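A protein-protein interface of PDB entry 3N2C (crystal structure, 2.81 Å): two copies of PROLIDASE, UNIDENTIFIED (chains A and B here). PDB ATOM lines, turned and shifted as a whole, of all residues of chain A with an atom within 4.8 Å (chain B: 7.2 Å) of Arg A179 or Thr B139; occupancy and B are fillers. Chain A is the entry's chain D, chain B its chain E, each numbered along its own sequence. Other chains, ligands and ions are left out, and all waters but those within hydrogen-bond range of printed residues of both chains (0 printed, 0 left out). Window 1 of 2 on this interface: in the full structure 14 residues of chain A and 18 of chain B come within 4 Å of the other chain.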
ATOM      1  N   ARG A 175      19.135 -20.816 -10.782  1.00  0.00           N
ATOM      2  CA  ARG A 175      18.425 -19.784 -11.543  1.00  0.00           C
ATOM      3  C   ARG A 175      18.946 -18.410 -11.174  1.00  0.00           C
ATOM      4  O   ARG A 175      19.253 -17.613 -12.058  1.00  0.00           O
ATOM      5  CB  ARG A 175      16.912 -19.834 -11.327  1.00  0.00           C
ATOM      6  CG  ARG A 175      16.178 -20.725 -12.304  1.00  0.00           C
ATOM      7  CD  ARG A 175      14.804 -20.172 -12.622  1.00  0.00           C
ATOM      8  NE  ARG A 175      13.761 -20.706 -11.751  1.00  0.00           N
ATOM      9  CZ  ARG A 175      12.964 -21.725 -12.072  1.00  0.00           C
ATOM     10  NH1 ARG A 175      12.035 -22.143 -11.220  1.00  0.00           N
ATOM     11  NH2 ARG A 175      13.095 -22.329 -13.248  1.00  0.00           N
ATOM     12  N   LEU A 176      19.073 -18.161  -9.872  1.00  0.00           N
ATOM     13  CA  LEU A 176      19.614 -16.904  -9.369  1.00  0.00           C
ATOM     14  C   LEU A 176      21.062 -16.701  -9.799  1.00  0.00           C
ATOM     15  O   LEU A 176      21.450 -15.594 -10.174  1.00  0.00           O
ATOM     16  CB  LEU A 176      19.498 -16.835  -7.847  1.00  0.00           C
ATOM     17  CG  LEU A 176      19.899 -15.521  -7.172  1.00  0.00           C
ATOM     18  CD1 LEU A 176      18.988 -14.393  -7.606  1.00  0.00           C
ATOM     19  CD2 LEU A 176      19.887 -15.666  -5.659  1.00  0.00           C
ATOM     20  N   ALA A 177      21.839 -17.782  -9.758  1.00  0.00           N
ATOM     21  CA  ALA A 177      23.242 -17.770 -10.172  1.00  0.00           C
ATOM     22  C   ALA A 177      23.417 -17.397 -11.643  1.00  0.00           C
ATOM     23  O   ALA A 177      24.269 -16.572 -11.965  1.00  0.00           O
ATOM     24  CB  ALA A 177      23.896 -19.116  -9.877  1.00  0.00           C
ATOM     25  N   VAL A 178      22.605 -17.997 -12.518  1.00  0.00           N
ATOM     26  CA  VAL A 178      22.634 -17.698 -13.955  1.00  0.00           C
ATOM     27  C   VAL A 178      22.220 -16.248 -14.234  1.00  0.00           C
ATOM     28  O   VAL A 178      22.860 -15.546 -15.022  1.00  0.00           O
ATOM     29  CB  VAL A 178      21.773 -18.692 -14.770  1.00  0.00           C
ATOM     30  CG1 VAL A 178      21.680 -18.277 -16.237  1.00  0.00           C
ATOM     31  CG2 VAL A 178      22.370 -20.066 -14.694  1.00  0.00           C
ATOM     32  N   ARG A 179      21.171 -15.797 -13.559  1.00  0.00           N
ATOM     33  CA  ARG A 179      20.760 -14.403 -13.624  1.00  0.00           C
ATOM     34  C   ARG A 179      21.859 -13.440 -13.156  1.00  0.00           C
ATOM     35  O   ARG A 179      22.062 -12.387 -13.766  1.00  0.00           O
ATOM     36  CB  ARG A 179      19.457 -14.196 -12.847  1.00  0.00           C
ATOM     37  CG  ARG A 179      18.262 -14.774 -13.576  1.00  0.00           C
ATOM     38  CD  ARG A 179      17.009 -14.827 -12.735  1.00  0.00           C
ATOM     39  NE  ARG A 179      16.000 -15.663 -13.385  1.00  0.00           N
ATOM     40  CZ  ARG A 179      14.786 -15.913 -12.902  1.00  0.00           C
ATOM     41  NH1 ARG A 179      14.390 -15.392 -11.747  1.00  0.00           N
ATOM     42  NH2 ARG A 179      13.962 -16.691 -13.585  1.00  0.00           N
ATOM     43  N   GLU A 180      22.579 -13.818 -12.100  1.00  0.00           N
ATOM     44  CA  GLU A 180      23.699 -13.018 -11.603  1.00  0.00           C
ATOM     45  C   GLU A 180      24.826 -12.909 -12.622  1.00  0.00           C
ATOM     46  O   GLU A 180      25.305 -11.806 -12.893  1.00  0.00           O
ATOM     47  CB  GLU A 180      24.242 -13.582 -10.291  1.00  0.00           C
ATOM     48  CG  GLU A 180      23.462 -13.155  -9.066  1.00  0.00           C
ATOM     49  CD  GLU A 180      23.707 -14.048  -7.864  1.00  0.00           C
ATOM     50  OE1 GLU A 180      22.908 -13.983  -6.905  1.00  0.00           O
ATOM     51  OE2 GLU A 180      24.692 -14.815  -7.873  1.00  0.00           O
ATOM     52  N   GLU A 181      25.225 -14.046 -13.195  1.00  0.00           N
ATOM     53  CA  GLU A 181      26.344 -14.091 -14.141  1.00  0.00           C
ATOM     54  C   GLU A 181      26.062 -13.344 -15.449  1.00  0.00           C
ATOM     55  O   GLU A 181      26.965 -12.735 -16.032  1.00  0.00           O
ATOM     56  CB  GLU A 181      26.772 -15.534 -14.423  1.00  0.00           C
ATOM     57  CG  GLU A 181      27.338 -16.267 -13.205  1.00  0.00           C
ATOM     58  CD  GLU A 181      28.468 -15.523 -12.496  1.00  0.00           C
ATOM     59  OE1 GLU A 181      29.498 -15.215 -13.133  1.00  0.00           O
ATOM     60  OE2 GLU A 181      28.328 -15.264 -11.284  1.00  0.00           O
ATOM     61  N   ILE A 182      24.806 -13.377 -15.883  1.00  0.00           N
ATOM     62  CA  ILE A 182      24.385 -12.697 -17.097  1.00  0.00           C
ATOM     63  C   ILE A 182      24.390 -11.170 -16.932  1.00  0.00           C
ATOM     64  O   ILE A 182      24.867 -10.447 -17.818  1.00  0.00           O
ATOM     65  CB  ILE A 182      23.042 -13.273 -17.620  1.00  0.00           C
ATOM     66  CG1 ILE A 182      23.334 -14.338 -18.683  1.00  0.00           C
ATOM     67  CG2 ILE A 182      22.141 -12.194 -18.211  1.00  0.00           C
ATOM     68  CD1 ILE A 182      22.343 -15.480 -18.725  1.00  0.00           C
ATOM     69  N   GLN A 183      23.920 -10.689 -15.783  1.00  0.00           N
ATOM     70  CA  GLN A 183      23.891  -9.252 -15.530  1.00  0.00           C
ATOM     71  C   GLN A 183      25.295  -8.717 -15.255  1.00  0.00           C
ATOM     72  O   GLN A 183      25.555  -7.534 -15.457  1.00  0.00           O
ATOM     73  CB  GLN A 183      22.892  -8.896 -14.417  1.00  0.00           C
ATOM     74  CG  GLN A 183      23.473  -8.604 -13.034  1.00  0.00           C
ATOM     75  CD  GLN A 183      23.718  -7.116 -12.790  1.00  0.00           C
ATOM     76  OE1 GLN A 183      22.806  -6.299 -12.899  1.00  0.00           O
ATOM     77  NE2 GLN A 183      24.954  -6.767 -12.447  1.00  0.00           N
ATOM     78  N   GLU A 220      17.440 -20.715 -18.356  1.00  0.00           N
ATOM     79  CA  GLU A 220      17.771 -19.341 -17.983  1.00  0.00           C
ATOM     80  C   GLU A 220      18.838 -18.770 -18.890  1.00  0.00           C
ATOM     81  O   GLU A 220      18.916 -17.552 -19.081  1.00  0.00           O
ATOM     82  CB  GLU A 220      18.198 -19.247 -16.525  1.00  0.00           C
ATOM     83  CG  GLU A 220      17.033 -19.169 -15.563  1.00  0.00           C
ATOM     84  CD  GLU A 220      16.154 -17.953 -15.787  1.00  0.00           C
ATOM     85  OE1 GLU A 220      16.690 -16.824 -15.815  1.00  0.00           O
ATOM     86  OE2 GLU A 220      14.924 -18.126 -15.927  1.00  0.00           O
ATOM     87  N   SER B 137      10.212  -7.952 -10.516  1.00  0.00           N
ATOM     88  CA  SER B 137      11.272  -8.154 -11.482  1.00  0.00           C
ATOM     89  C   SER B 137      12.221  -9.246 -11.016  1.00  0.00           C
ATOM     90  O   SER B 137      12.341  -9.506  -9.817  1.00  0.00           O
ATOM     91  CB  SER B 137      12.046  -6.856 -11.678  1.00  0.00           C
ATOM     92  OG  SER B 137      13.023  -6.995 -12.698  1.00  0.00           O
ATOM     93  N   GLN B 138      12.881  -9.892 -11.970  1.00  0.00           N
ATOM     94  CA  GLN B 138      13.915 -10.865 -11.649  1.00  0.00           C
ATOM     95  C   GLN B 138      15.264 -10.165 -11.524  1.00  0.00           C
ATOM     96  O   GLN B 138      15.355  -8.956 -11.726  1.00  0.00           O
ATOM     97  CB  GLN B 138      13.977 -11.953 -12.716  1.00  0.00           C
ATOM     98  CG  GLN B 138      14.160 -11.435 -14.125  1.00  0.00           C
ATOM     99  CD  GLN B 138      14.871 -12.434 -15.004  1.00  0.00           C
ATOM    100  OE1 GLN B 138      14.240 -13.275 -15.639  1.00  0.00           O
ATOM    101  NE2 GLN B 138      16.198 -12.363 -15.031  1.00  0.00           N
ATOM    102  N   THR B 139      16.302 -10.925 -11.183  1.00  0.00           N
ATOM    103  CA  THR B 139      17.654 -10.385 -11.079  1.00  0.00           C
ATOM    104  C   THR B 139      18.215 -10.136 -12.472  1.00  0.00           C
ATOM    105  O   THR B 139      18.094 -10.984 -13.361  1.00  0.00           O
ATOM    106  CB  THR B 139      18.575 -11.308 -10.267  1.00  0.00           C
ATOM    107  OG1 THR B 139      18.068 -11.413  -8.930  1.00  0.00           O
ATOM    108  CG2 THR B 139      19.995 -10.759 -10.214  1.00  0.00           C
ATOM    109  N   GLY B 140      18.791  -8.947 -12.658  1.00  0.00           N
ATOM    110  CA  GLY B 140      19.246  -8.488 -13.961  1.00  0.00           C
ATOM    111  C   GLY B 140      18.061  -8.188 -14.853  1.00  0.00           C
ATOM    112  O   GLY B 140      18.192  -8.095 -16.074  1.00  0.00           O
ATOM    113  N   GLY B 141      16.900  -8.039 -14.227  1.00  0.00           N
ATOM    114  CA  GLY B 141      15.660  -7.814 -14.937  1.00  0.00           C
ATOM    115  C   GLY B 141      15.410  -6.354 -15.248  1.00  0.00           C
ATOM    116  O   GLY B 141      16.268  -5.492 -15.020  1.00  0.00           O
ATOM    117  N   HIS B 142      14.212  -6.081 -15.755  1.00  0.00           N
ATOM    118  CA  HIS B 142      13.820  -4.743 -16.158  1.00  0.00           C
ATOM    119  C   HIS B 142      13.599  -3.804 -14.961  1.00  0.00           C
ATOM    120  O   HIS B 142      13.513  -2.584 -15.119  1.00  0.00           O
ATOM    121  CB  HIS B 142      12.588  -4.812 -17.067  1.00  0.00           C
ATOM    122  CG  HIS B 142      12.215  -3.498 -17.680  1.00  0.00           C
ATOM    123  ND1 HIS B 142      13.151  -2.608 -18.164  1.00  0.00           N
ATOM    124  CD2 HIS B 142      11.007  -2.920 -17.880  1.00  0.00           C
ATOM    125  CE1 HIS B 142      12.537  -1.536 -18.626  1.00  0.00           C
ATOM    126  NE2 HIS B 142      11.235  -1.704 -18.475  1.00  0.00           N
ATOM    127  N   ASP B 144      15.705  -4.412 -12.127  1.00  0.00           N
ATOM    128  CA  ASP B 144      17.016  -4.418 -11.490  1.00  0.00           C
ATOM    129  C   ASP B 144      17.862  -3.303 -12.087  1.00  0.00           C
ATOM    130  O   ASP B 144      18.482  -3.477 -13.137  1.00  0.00           O
ATOM    131  CB  ASP B 144      17.704  -5.776 -11.664  1.00  0.00           C
ATOM    132  CG  ASP B 144      18.825  -6.008 -10.654  1.00  0.00           C
ATOM    133  OD1 ASP B 144      19.445  -5.032 -10.185  1.00  0.00           O
ATOM    134  OD2 ASP B 144      19.097  -7.183 -10.326  1.00  0.00           O
ATOM    135  N   ARG B 146      20.584  -1.968 -10.919  1.00  0.00           N
ATOM    136  CA  ARG B 146      21.997  -2.043 -10.575  1.00  0.00           C
ATOM    137  C   ARG B 146      22.824  -2.036 -11.855  1.00  0.00           C
ATOM    138  O   ARG B 146      22.390  -2.595 -12.871  1.00  0.00           O
ATOM    139  CB  ARG B 146      22.284  -3.310  -9.771  1.00  0.00           C
ATOM    140  CG  ARG B 146      21.819  -3.245  -8.338  1.00  0.00           C
ATOM    141  CD  ARG B 146      22.052  -4.560  -7.632  1.00  0.00           C
ATOM    142  NE  ARG B 146      20.988  -5.519  -7.906  1.00  0.00           N
ATOM    143  CZ  ARG B 146      20.699  -6.566  -7.139  1.00  0.00           C
ATOM    144  NH1 ARG B 146      21.396  -6.806  -6.036  1.00  0.00           N
ATOM    145  NH2 ARG B 146      19.711  -7.381  -7.483  1.00  0.00           N
ATOM    146  N   LEU B 151      26.791  -6.950  -7.381  1.00  0.00           N
ATOM    147  CA  LEU B 151      25.449  -7.227  -6.867  1.00  0.00           C
ATOM    148  C   LEU B 151      25.407  -7.378  -5.345  1.00  0.00           C
ATOM    149  O   LEU B 151      25.577  -8.482  -4.817  1.00  0.00           O
ATOM    150  CB  LEU B 151      24.876  -8.481  -7.541  1.00  0.00           C
ATOM    151  CG  LEU B 151      24.575  -8.404  -9.042  1.00  0.00           C
ATOM    152  CD1 LEU B 151      24.769  -9.745  -9.701  1.00  0.00           C
ATOM    153  CD2 LEU B 151      23.176  -7.894  -9.291  1.00  0.00           C
ATOM    154  N   VAL B 167      12.981  -6.656  -6.667  1.00  0.00           N
ATOM    155  CA  VAL B 167      13.668  -7.793  -7.265  1.00  0.00           C
ATOM    156  C   VAL B 167      13.446  -9.072  -6.448  1.00  0.00           C
ATOM    157  O   VAL B 167      13.922  -9.193  -5.316  1.00  0.00           O
ATOM    158  CB  VAL B 167      15.174  -7.498  -7.421  1.00  0.00           C
ATOM    159  CG1 VAL B 167      15.884  -8.637  -8.136  1.00  0.00           C
ATOM    160  CG2 VAL B 167      15.380  -6.191  -8.166  1.00  0.00           C
ATOM    161  N   VAL B 168      12.702 -10.015  -7.022  1.00  0.00           N
ATOM    162  CA  VAL B 168      12.468 -11.320  -6.398  1.00  0.00           C
ATOM    163  C   VAL B 168      12.566 -12.443  -7.420  1.00  0.00           C
ATOM    164  O   VAL B 168      12.018 -12.345  -8.511  1.00  0.00           O
ATOM    165  CB  VAL B 168      11.102 -11.406  -5.675  1.00  0.00           C
ATOM    166  CG1 VAL B 168      11.204 -10.855  -4.255  1.00  0.00           C
ATOM    167  CG2 VAL B 168      10.016 -10.688  -6.465  1.00  0.00           C
ATOM    168  N   ASP B 169      13.278 -13.505  -7.059  1.00  0.00           N
ATOM    169  CA  ASP B 169      13.473 -14.647  -7.942  1.00  0.00           C
ATOM    170  C   ASP B 169      12.936 -15.906  -7.298  1.00  0.00           C
ATOM    171  O   ASP B 169      12.971 -16.056  -6.077  1.00  0.00           O
ATOM    172  CB  ASP B 169      14.958 -14.865  -8.235  1.00  0.00           C
ATOM    173  CG  ASP B 169      15.661 -13.611  -8.706  1.00  0.00           C
ATOM    174  OD1 ASP B 169      15.941 -13.516  -9.920  1.00  0.00           O
ATOM    175  OD2 ASP B 169      15.948 -12.735  -7.857  1.00  0.00           O
ATOM    176  N   GLY B 170      12.458 -16.821  -8.129  1.00  0.00           N
ATOM    177  CA  GLY B 170      12.078 -18.143  -7.662  1.00  0.00           C
ATOM    178  C   GLY B 170      10.616 -18.278  -7.332  1.00  0.00           C
ATOM    179  O   GLY B 170       9.997 -17.312  -6.901  1.00  0.00           O
ATOM    180  N   VAL B 174       8.617 -15.502  -5.337  1.00  0.00           N
ATOM    181  CA  VAL B 174       7.623 -14.621  -5.960  1.00  0.00           C
ATOM    182  C   VAL B 174       6.230 -14.854  -5.410  1.00  0.00           C
ATOM    183  O   VAL B 174       5.403 -13.950  -5.453  1.00  0.00           O
ATOM    184  CB  VAL B 174       7.593 -14.686  -7.525  1.00  0.00           C
ATOM    185  CG1 VAL B 174       8.950 -14.316  -8.116  1.00  0.00           C
ATOM    186  CG2 VAL B 174       7.106 -16.044  -8.036  1.00  0.00           C
ATOM    187  N   THR B 201      20.975  -3.204 -17.861  1.00  0.00           N
ATOM    188  CA  THR B 201      21.616  -4.484 -18.215  1.00  0.00           C
ATOM    189  C   THR B 201      20.946  -5.312 -19.325  1.00  0.00           C
ATOM    190  O   THR B 201      21.638  -6.012 -20.069  1.00  0.00           O
ATOM    191  CB  THR B 201      21.842  -5.391 -16.972  1.00  0.00           C
ATOM    192  OG1 THR B 201      20.582  -5.809 -16.433  1.00  0.00           O
ATOM    193  CG2 THR B 201      22.645  -4.663 -15.901  1.00  0.00           C
ATOM    194  N   GLN B 208      11.975 -12.516 -19.609  1.00  0.00           N
ATOM    195  CA  GLN B 208      12.287 -12.546 -18.183  1.00  0.00           C
ATOM    196  C   GLN B 208      11.254 -13.336 -17.386  1.00  0.00           C
ATOM    197  O   GLN B 208      10.096 -13.421 -17.790  1.00  0.00           O
ATOM    198  CB  GLN B 208      12.443 -11.130 -17.635  1.00  0.00           C
ATOM    199  CG  GLN B 208      13.779 -10.495 -17.990  1.00  0.00           C
ATOM    200  CD  GLN B 208      13.832  -9.025 -17.668  1.00  0.00           C
ATOM    201  OE1 GLN B 208      13.011  -8.511 -16.909  1.00  0.00           O
ATOM    202  NE2 GLN B 208      14.802  -8.333 -18.245  1.00  0.00           N
ATOM    203  N   TYR B 209      11.696 -13.898 -16.255  1.00  0.00           N
ATOM    204  CA  TYR B 209      10.962 -14.903 -15.450  1.00  0.00           C
ATOM    205  C   TYR B 209      10.699 -16.226 -16.173  1.00  0.00           C
ATOM    206  O   TYR B 209      10.430 -16.258 -17.372  1.00  0.00           O
ATOM    207  CB  TYR B 209       9.652 -14.361 -14.862  1.00  0.00           C
ATOM    208  CG  TYR B 209       9.804 -13.569 -13.587  1.00  0.00           C
ATOM    209  CD1 TYR B 209       9.108 -12.378 -13.400  1.00  0.00           C
ATOM    210  CD2 TYR B 209      10.642 -14.007 -12.566  1.00  0.00           C
ATOM    211  CE1 TYR B 209       9.239 -11.649 -12.231  1.00  0.00           C
ATOM    212  CE2 TYR B 209      10.784 -13.287 -11.397  1.00  0.00           C
ATOM    213  CZ  TYR B 209      10.081 -12.110 -11.232  1.00  0.00           C
ATOM    214  OH  TYR B 209      10.216 -11.393 -10.065  1.00  0.00           O
ATOM    215  N   SER B 210      10.779 -17.323 -15.428  1.00  0.00           N
ATOM    216  CA  SER B 210      10.462 -18.634 -15.977  1.00  0.00           C
ATOM    217  C   SER B 210       8.955 -18.784 -16.044  1.00  0.00           C
ATOM    218  O   SER B 210       8.227 -17.989 -15.452  1.00  0.00           O
ATOM    219  CB  SER B 210      11.056 -19.736 -15.106  1.00  0.00           C
ATOM    220  OG  SER B 210      10.444 -19.753 -13.829  1.00  0.00           O
ATOM    221  N   GLU B 211       8.489 -19.801 -16.765  1.00  0.00           N
ATOM    222  CA  GLU B 211       7.057 -20.082 -16.849  1.00  0.00           C
ATOM    223  C   GLU B 211       6.511 -20.511 -15.491  1.00  0.00           C
ATOM    224  O   GLU B 211       5.386 -20.158 -15.141  1.00  0.00           O
ATOM    225  CB  GLU B 211       6.762 -21.140 -17.909  1.00  0.00           C
ATOM    226  CG  GLU B 211       6.997 -20.672 -19.336  1.00  0.00           C
ATOM    227  CD  GLU B 211       6.113 -21.387 -20.344  1.00  0.00           C
ATOM    228  OE1 GLU B 211       6.394 -21.286 -21.557  1.00  0.00           O
ATOM    229  OE2 GLU B 211       5.131 -22.045 -19.932  1.00  0.00           O
ATOM    230  N   GLU B 213       7.521 -19.355 -12.622  1.00  0.00           N
ATOM    231  CA  GLU B 213       7.370 -18.150 -11.824  1.00  0.00           C
ATOM    232  C   GLU B 213       6.138 -17.342 -12.197  1.00  0.00           C
ATOM    233  O   GLU B 213       5.430 -16.868 -11.312  1.00  0.00           O
ATOM    234  CB  GLU B 213       8.618 -17.281 -11.919  1.00  0.00           C
ATOM    235  CG  GLU B 213       9.792 -17.791 -11.098  1.00  0.00           C
ATOM    236  CD  GLU B 213      11.111 -17.249 -11.596  1.00  0.00           C
ATOM    237  OE1 GLU B 213      11.930 -16.808 -10.763  1.00  0.00           O
ATOM    238  OE2 GLU B 213      11.323 -17.241 -12.826  1.00  0.00           O
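The guanidinium group (NH1) of Arg A179 lies within salt-bridge range of the side-chain carboxylate (OD1) of Asp B169, at 3.0 Å.
The guanidinium group (NH2) of Arg A179 is in salt-bridge range of the side-chain carboxylate (OE2) of Glu B213 (2.8 Å).
The backbone carbonyl oxygen (O) of Ser B137 sits at hydrogen-bond distance from the side-chain hydroxyl (OH) of Tyr B209, at 2.9 Å.
The side-chain amide oxygen (OE1) of Gln B138 is in hydrogen-bond range of the backbone NH (N) of Tyr B209, 2.7 Å away.
The backbone NH (N) of Gly B140 lies within hydrogen-bond range of the side-chain carboxylate (OD2) of Asp B144, 2.9 Å away.
The side-chain carboxylate of Asp B144 lies within salt-bridge range of the guanidinium group of Arg B146 (2.8 Å).
The side-chain hydroxyl (OH) of Tyr B209 is in hydrogen-bond range of the backbone carbonyl oxygen (O) of Val B168 (2.6 Å).
The side-chain carboxylate of Glu B213 lies within hydrogen-bond range of the backbone NH of Ser B210, at 2.7 Å.
OG1 of Thr B139 touches CD1 of Leu A176 (3.4 Å).
Leu A176 touches Asp B169.
Arg A179 touches Gln B138.
CB of Arg A179 touches O of Thr B139, at 3.5 Å.
Tyr B209 touches Arg A179.
Arg A179 touches Ser B210 (NH2 to N, 3.7 Å).
Leu B151 touches Glu A180 (CD1 to CG, 3.7 Å).
CB of Gln A183 touches CA of Gly B140, 3.7 Å away.
Gln A183 touches Arg B146.
Gln A183 touches Leu B151.
Arg A179 touches just these residues of chain B: Gln B138, Thr B139, Asp B169, Tyr B209, Ser B210 and Glu B213.
Thr B139 touches just these residues of chain A: Leu A176 (3.4 Å) and Arg A179 (3.5 Å).
Printed residues of chain A within 4 Å of Asp B169: Leu A176 and Arg A179.
Of the printed residues of chain A, Tyr B209 touches Arg A179.
Printed residues of chain B within 4 Å of Leu A176: Thr B139 (3.4 Å) and Asp B169 (3.5 Å).
Printed residues of chain B within 4 Å of Gln A183: Gly B140, Arg B146, Leu B151 and Thr B201.
The nearest residue of chain B that does not touch Arg A179 is Gly B170 (4.3 Å).
The nearest residue of chain A that does not touch Thr B139 is Glu A180 (4.4 Å).
Of the 20 printed residues of chain B, 10 touch a printed residue of chain A.
Of the 10 printed residues of chain A, 5 touch a printed residue of chain B.
Hydrophobic or aromatic side chains of chain A that line the printed part of chain B: Leu A176.
Along chain A the printed residues that touch a printed residue of chain B span positions 175 to 183.
Among the printed residues, 14 pairs touch across the chains.
No position is printed for both chains.
Of the 14 pairs that touch across the chains among the printed residues, none has its exchanged pair printed and touching as well.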
